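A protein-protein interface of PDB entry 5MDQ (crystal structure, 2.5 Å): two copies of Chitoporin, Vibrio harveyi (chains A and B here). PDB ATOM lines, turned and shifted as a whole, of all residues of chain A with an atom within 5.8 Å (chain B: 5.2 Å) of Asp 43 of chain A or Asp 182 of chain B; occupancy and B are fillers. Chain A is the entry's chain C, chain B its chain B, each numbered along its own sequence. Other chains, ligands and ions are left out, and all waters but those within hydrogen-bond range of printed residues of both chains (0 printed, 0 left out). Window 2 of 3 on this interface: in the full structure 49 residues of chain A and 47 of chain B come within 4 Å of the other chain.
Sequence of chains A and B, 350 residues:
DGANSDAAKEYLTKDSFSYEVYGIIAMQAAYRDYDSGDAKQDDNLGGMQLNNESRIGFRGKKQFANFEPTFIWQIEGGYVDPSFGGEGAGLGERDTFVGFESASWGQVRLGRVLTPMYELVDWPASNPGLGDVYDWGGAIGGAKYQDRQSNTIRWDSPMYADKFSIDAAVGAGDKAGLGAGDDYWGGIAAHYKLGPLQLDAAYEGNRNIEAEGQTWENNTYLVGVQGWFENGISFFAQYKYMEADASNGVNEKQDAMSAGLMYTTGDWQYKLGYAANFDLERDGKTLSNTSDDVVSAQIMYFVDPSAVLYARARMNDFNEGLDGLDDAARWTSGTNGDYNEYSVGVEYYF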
ATOM      1  N   ASP A  38       5.065   3.810  -7.273  1.00  0.00           N
ATOM      2  CA  ASP A  38       5.756   3.836  -8.586  1.00  0.00           C
ATOM      3  C   ASP A  38       5.979   5.310  -9.018  1.00  0.00           C
ATOM      4  O   ASP A  38       5.005   6.070  -9.163  1.00  0.00           O
ATOM      5  CB  ASP A  38       4.868   3.112  -9.581  1.00  0.00           C
ATOM      6  CG  ASP A  38       5.467   3.000 -10.974  1.00  0.00           C
ATOM      7  OD1 ASP A  38       6.360   3.743 -11.395  1.00  0.00           O
ATOM      8  OD2 ASP A  38       4.958   2.137 -11.697  1.00  0.00           O
ATOM      9  N   ALA A  39       7.245   5.725  -9.184  1.00  0.00           N
ATOM     10  CA  ALA A  39       7.576   7.153  -9.441  1.00  0.00           C
ATOM     11  C   ALA A  39       7.046   7.649 -10.778  1.00  0.00           C
ATOM     12  O   ALA A  39       6.642   8.814 -10.910  1.00  0.00           O
ATOM     13  CB  ALA A  39       9.064   7.403  -9.363  1.00  0.00           C
ATOM     14  N   LYS A  40       7.011   6.752 -11.754  1.00  0.00           N
ATOM     15  CA  LYS A  40       6.439   7.049 -13.082  1.00  0.00           C
ATOM     16  C   LYS A  40       4.930   7.331 -12.985  1.00  0.00           C
ATOM     17  O   LYS A  40       4.433   8.357 -13.482  1.00  0.00           O
ATOM     18  CB  LYS A  40       6.755   5.879 -14.009  1.00  0.00           C
ATOM     19  CG  LYS A  40       6.272   5.988 -15.437  1.00  0.00           C
ATOM     20  CD  LYS A  40       6.795   7.232 -16.152  1.00  0.00           C
ATOM     21  CE  LYS A  40       6.256   7.263 -17.579  1.00  0.00           C
ATOM     22  NZ  LYS A  40       5.946   8.628 -18.075  1.00  0.00           N
ATOM     23  N   GLN A  41       4.205   6.443 -12.316  1.00  0.00           N
ATOM     24  CA  GLN A  41       2.785   6.638 -12.124  1.00  0.00           C
ATOM     25  C   GLN A  41       2.502   7.925 -11.396  1.00  0.00           C
ATOM     26  O   GLN A  41       1.529   8.602 -11.668  1.00  0.00           O
ATOM     27  CB  GLN A  41       2.199   5.416 -11.411  1.00  0.00           C
ATOM     28  CG  GLN A  41       0.677   5.286 -11.432  1.00  0.00           C
ATOM     29  CD  GLN A  41       0.174   4.216 -10.424  1.00  0.00           C
ATOM     30  OE1 GLN A  41       0.634   3.068 -10.439  1.00  0.00           O
ATOM     31  NE2 GLN A  41      -0.721   4.619  -9.490  1.00  0.00           N
ATOM     32  N   ASP A  42       3.375   8.288 -10.468  1.00  0.00           N
ATOM     33  CA  ASP A  42       3.230   9.534  -9.697  1.00  0.00           C
ATOM     34  C   ASP A  42       3.365  10.811 -10.502  1.00  0.00           C
ATOM     35  O   ASP A  42       2.639  11.772 -10.261  1.00  0.00           O
ATOM     36  CB  ASP A  42       4.287   9.603  -8.607  1.00  0.00           C
ATOM     37  CG  ASP A  42       4.101   8.573  -7.504  1.00  0.00           C
ATOM     38  OD1 ASP A  42       2.966   8.109  -7.240  1.00  0.00           O
ATOM     39  OD2 ASP A  42       5.129   8.280  -6.836  1.00  0.00           O
ATOM     40  N   ASP A  43       4.324  10.824 -11.426  1.00  0.00           N
ATOM     41  CA  ASP A  43       4.428  11.897 -12.434  1.00  0.00           C
ATOM     42  C   ASP A  43       3.239  11.980 -13.401  1.00  0.00           C
ATOM     43  O   ASP A  43       2.750  13.082 -13.767  1.00  0.00           O
ATOM     44  CB  ASP A  43       5.651  11.698 -13.297  1.00  0.00           C
ATOM     45  CG  ASP A  43       6.913  11.790 -12.543  1.00  0.00           C
ATOM     46  OD1 ASP A  43       6.971  12.365 -11.426  1.00  0.00           O
ATOM     47  OD2 ASP A  43       7.912  11.296 -13.099  1.00  0.00           O
ATOM     48  N   ASN A  44       2.768  10.828 -13.861  1.00  0.00           N
ATOM     49  CA  ASN A  44       1.633  10.866 -14.768  1.00  0.00           C
ATOM     50  C   ASN A  44       0.460  11.554 -14.097  1.00  0.00           C
ATOM     51  O   ASN A  44       0.061  12.680 -14.517  1.00  0.00           O
ATOM     52  CB  ASN A  44       1.342   9.494 -15.295  1.00  0.00           C
ATOM     53  CG  ASN A  44       2.511   8.937 -16.097  1.00  0.00           C
ATOM     54  OD1 ASN A  44       3.406   9.663 -16.540  1.00  0.00           O
ATOM     55  ND2 ASN A  44       2.481   7.667 -16.350  1.00  0.00           N
ATOM     56  N   LEU A  45       0.054  10.989 -12.962  1.00  0.00           N
ATOM     57  CA  LEU A  45      -1.208  11.385 -12.299  1.00  0.00           C
ATOM     58  C   LEU A  45      -1.142  12.702 -11.593  1.00  0.00           C
ATOM     59  O   LEU A  45      -2.133  13.439 -11.518  1.00  0.00           O
ATOM     60  CB  LEU A  45      -1.656  10.328 -11.311  1.00  0.00           C
ATOM     61  CG  LEU A  45      -1.915   8.918 -11.840  1.00  0.00           C
ATOM     62  CD1 LEU A  45      -1.786   7.895 -10.748  1.00  0.00           C
ATOM     63  CD2 LEU A  45      -3.283   8.845 -12.448  1.00  0.00           C
ATOM     64  N   GLY A  46       0.042  12.988 -11.070  1.00  0.00           N
ATOM     65  CA  GLY A  46       0.288  14.239 -10.394  1.00  0.00           C
ATOM     66  C   GLY A  46       0.687  15.318 -11.345  1.00  0.00           C
ATOM     67  O   GLY A  46       0.856  15.068 -12.552  1.00  0.00           O
ATOM     68  N   GLY A  47       0.760  16.504 -10.777  1.00  0.00           N
ATOM     69  CA  GLY A  47       1.105  17.700 -11.465  1.00  0.00           C
ATOM     70  C   GLY A  47      -0.044  18.654 -11.354  1.00  0.00           C
ATOM     71  O   GLY A  47      -0.984  18.420 -10.621  1.00  0.00           O
ATOM     72  N   ALA B 176      -0.802  14.777 -19.888  1.00  0.00           N
ATOM     73  CA  ALA B 176      -0.944  15.326 -18.536  1.00  0.00           C
ATOM     74  C   ALA B 176      -2.403  15.623 -18.242  1.00  0.00           C
ATOM     75  O   ALA B 176      -2.890  15.352 -17.170  1.00  0.00           O
ATOM     76  CB  ALA B 176      -0.121  16.586 -18.406  1.00  0.00           C
ATOM     77  N   ALA B 180      -2.049  10.957 -17.466  1.00  0.00           N
ATOM     78  CA  ALA B 180      -1.331   9.888 -18.161  1.00  0.00           C
ATOM     79  C   ALA B 180       0.085  10.238 -18.549  1.00  0.00           C
ATOM     80  O   ALA B 180       0.729   9.414 -19.194  1.00  0.00           O
ATOM     81  CB  ALA B 180      -2.109   9.485 -19.410  1.00  0.00           C
ATOM     82  N   GLY B 181       0.594  11.408 -18.136  1.00  0.00           N
ATOM     83  CA  GLY B 181       1.970  11.814 -18.403  1.00  0.00           C
ATOM     84  C   GLY B 181       2.301  13.121 -17.729  1.00  0.00           C
ATOM     85  O   GLY B 181       1.472  13.702 -17.037  1.00  0.00           O
ATOM     86  N   ASP B 182       3.546  13.567 -17.926  1.00  0.00           N
ATOM     87  CA  ASP B 182       4.073  14.832 -17.341  1.00  0.00           C
ATOM     88  C   ASP B 182       4.631  15.797 -18.452  1.00  0.00           C
ATOM     89  O   ASP B 182       5.572  16.577 -18.223  1.00  0.00           O
ATOM     90  CB  ASP B 182       5.087  14.551 -16.234  1.00  0.00           C
ATOM     91  CG  ASP B 182       6.307  13.700 -16.697  1.00  0.00           C
ATOM     92  OD1 ASP B 182       6.424  13.495 -17.928  1.00  0.00           O
ATOM     93  OD2 ASP B 182       7.191  13.345 -15.793  1.00  0.00           O
ATOM     94  N   ASP B 183       3.980  15.759 -19.639  1.00  0.00           N
ATOM     95  CA  ASP B 183       4.229  16.738 -20.676  1.00  0.00           C
ATOM     96  C   ASP B 183       3.709  18.141 -20.313  1.00  0.00           C
ATOM     97  O   ASP B 183       2.728  18.314 -19.575  1.00  0.00           O
ATOM     98  CB  ASP B 183       3.766  16.263 -22.058  1.00  0.00           C
ATOM     99  CG  ASP B 183       2.301  15.745 -22.111  1.00  0.00           C
ATOM    100  OD1 ASP B 183       1.564  15.854 -21.133  1.00  0.00           O
ATOM    101  OD2 ASP B 183       1.880  15.264 -23.182  1.00  0.00           O
ATOM    102  N   TYR B 184       4.453  19.144 -20.779  1.00  0.00           N
ATOM    103  CA  TYR B 184       4.102  20.536 -20.549  1.00  0.00           C
ATOM    104  C   TYR B 184       4.777  21.357 -21.623  1.00  0.00           C
ATOM    105  O   TYR B 184       5.615  20.854 -22.411  1.00  0.00           O
ATOM    106  CB  TYR B 184       4.482  21.029 -19.125  1.00  0.00           C
ATOM    107  CG  TYR B 184       5.947  21.085 -18.858  1.00  0.00           C
ATOM    108  CD1 TYR B 184       6.642  19.942 -18.503  1.00  0.00           C
ATOM    109  CD2 TYR B 184       6.657  22.296 -18.962  1.00  0.00           C
ATOM    110  CE1 TYR B 184       8.001  19.962 -18.278  1.00  0.00           C
ATOM    111  CE2 TYR B 184       8.061  22.367 -18.718  1.00  0.00           C
ATOM    112  CZ  TYR B 184       8.716  21.179 -18.370  1.00  0.00           C
ATOM    113  OH  TYR B 184      10.058  21.112 -18.165  1.00  0.00           O
ATOM    114  N   ARG B 207       7.929  20.008 -23.633  1.00  0.00           N
ATOM    115  CA  ARG B 207       8.802  19.169 -22.852  1.00  0.00           C
ATOM    116  C   ARG B 207       8.023  17.919 -22.448  1.00  0.00           C
ATOM    117  O   ARG B 207       6.811  17.999 -22.248  1.00  0.00           O
ATOM    118  CB  ARG B 207       9.262  19.952 -21.605  1.00  0.00           C
ATOM    119  CG  ARG B 207       9.961  21.286 -21.888  1.00  0.00           C
ATOM    120  CD  ARG B 207      11.325  21.029 -22.485  1.00  0.00           C
ATOM    121  NE  ARG B 207      12.102  22.219 -22.834  1.00  0.00           N
ATOM    122  CZ  ARG B 207      12.127  22.807 -24.026  1.00  0.00           C
ATOM    123  NH1 ARG B 207      11.340  22.408 -25.008  1.00  0.00           N
ATOM    124  NH2 ARG B 207      12.902  23.817 -24.225  1.00  0.00           N
ATOM    125  N   ASN B 208       8.762  16.824 -22.278  1.00  0.00           N
ATOM    126  CA  ASN B 208       8.312  15.488 -21.905  1.00  0.00           C
ATOM    127  C   ASN B 208       7.246  14.912 -22.830  1.00  0.00           C
ATOM    128  O   ASN B 208       6.360  14.244 -22.396  1.00  0.00           O
ATOM    129  CB  ASN B 208       7.852  15.418 -20.479  1.00  0.00           C
ATOM    130  CG  ASN B 208       8.922  15.754 -19.481  1.00  0.00           C
ATOM    131  OD1 ASN B 208      10.011  15.169 -19.496  1.00  0.00           O
ATOM    132  ND2 ASN B 208       8.588  16.647 -18.540  1.00  0.00           N
ATOM    133  N   GLU B 210       6.024  12.252 -25.197  1.00  0.00           N
ATOM    134  CA  GLU B 210       6.300  10.865 -25.492  1.00  0.00           C
ATOM    135  C   GLU B 210       5.693  10.515 -26.861  1.00  0.00           C
ATOM    136  O   GLU B 210       4.593  10.851 -27.131  1.00  0.00           O
ATOM    137  CB  GLU B 210       5.720   9.979 -24.402  1.00  0.00           C
ATOM    138  CG  GLU B 210       6.574   9.914 -23.151  1.00  0.00           C
ATOM    139  CD  GLU B 210       5.834   9.321 -21.970  1.00  0.00           C
ATOM    140  OE1 GLU B 210       4.735   8.706 -22.165  1.00  0.00           O
ATOM    141  OE2 GLU B 210       6.343   9.452 -20.849  1.00  0.00           O
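The side-chain carboxylate of Glu 210 of chain B is in salt-bridge range of the side-chain amino group of Lys 40 of chain A (2.9 Å).
The side-chain carboxylate of Asp 182 of chain B lies close to the side-chain carboxylate of Asp 43 of chain A, at 3.5 Å.
The backbone carbonyl oxygen (O) of Asn 44 of chain A lies close to the backbone carbonyl oxygen (O) of Gly 181 of chain B (3.1 Å).
O of Asp 182 of chain B is in hydrogen-bond range of ND2 of Asn 208 of chain B (3.0 Å).
The side-chain carboxylate of Asp 38 of chain A is in hydrogen-bond range of the backbone NH of Lys 40 of chain A (3.1 Å).
NZ of Lys 40 of chain A lies within hydrogen-bond range of OD1 of Asn 44 of chain A (3.1 Å).
Asp 43 of chain A touches Gly 181 of chain B.
Ala 180 of chain B touches Asn 44 of chain A (C to CB, 3.6 Å).
Asp 43 of chain A touches two residues of chain B.
Of the printed residues of chain B, Lys 40 of chain A touches Glu 210.
Of the printed residues of chain B, Asn 44 of chain A touches Ala 180 (3.6 Å) and Gly 181 (3.1 Å).
Printed residues of chain A within 4 Å of Glu 210 of chain B: Lys 40.
Of the printed residues of chain A, Gly 181 of chain B touches Asp 43 and Asn 44.
The nearest printed residue of chain B that does not touch Asp 43 of chain A is Ala 180 of chain B (6.2 Å).
The nearest residue of chain A that does not touch Asp 182 of chain B is Asn 44 of chain A (4.1 Å).
The nearest printed residue of chain B that does not touch Asn 44 of chain A is Asp 182 of chain B (4.1 Å).
Among the printed residues, 5 pairs touch across the chains.
Among the printed residues, Asp or Glu carboxylates within 4 Å of a Lys or Arg side-chain nitrogen of the other chain: Lys 40 of chain A with Glu 210 of chain B (2.9 Å).
No position is printed for both chains.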
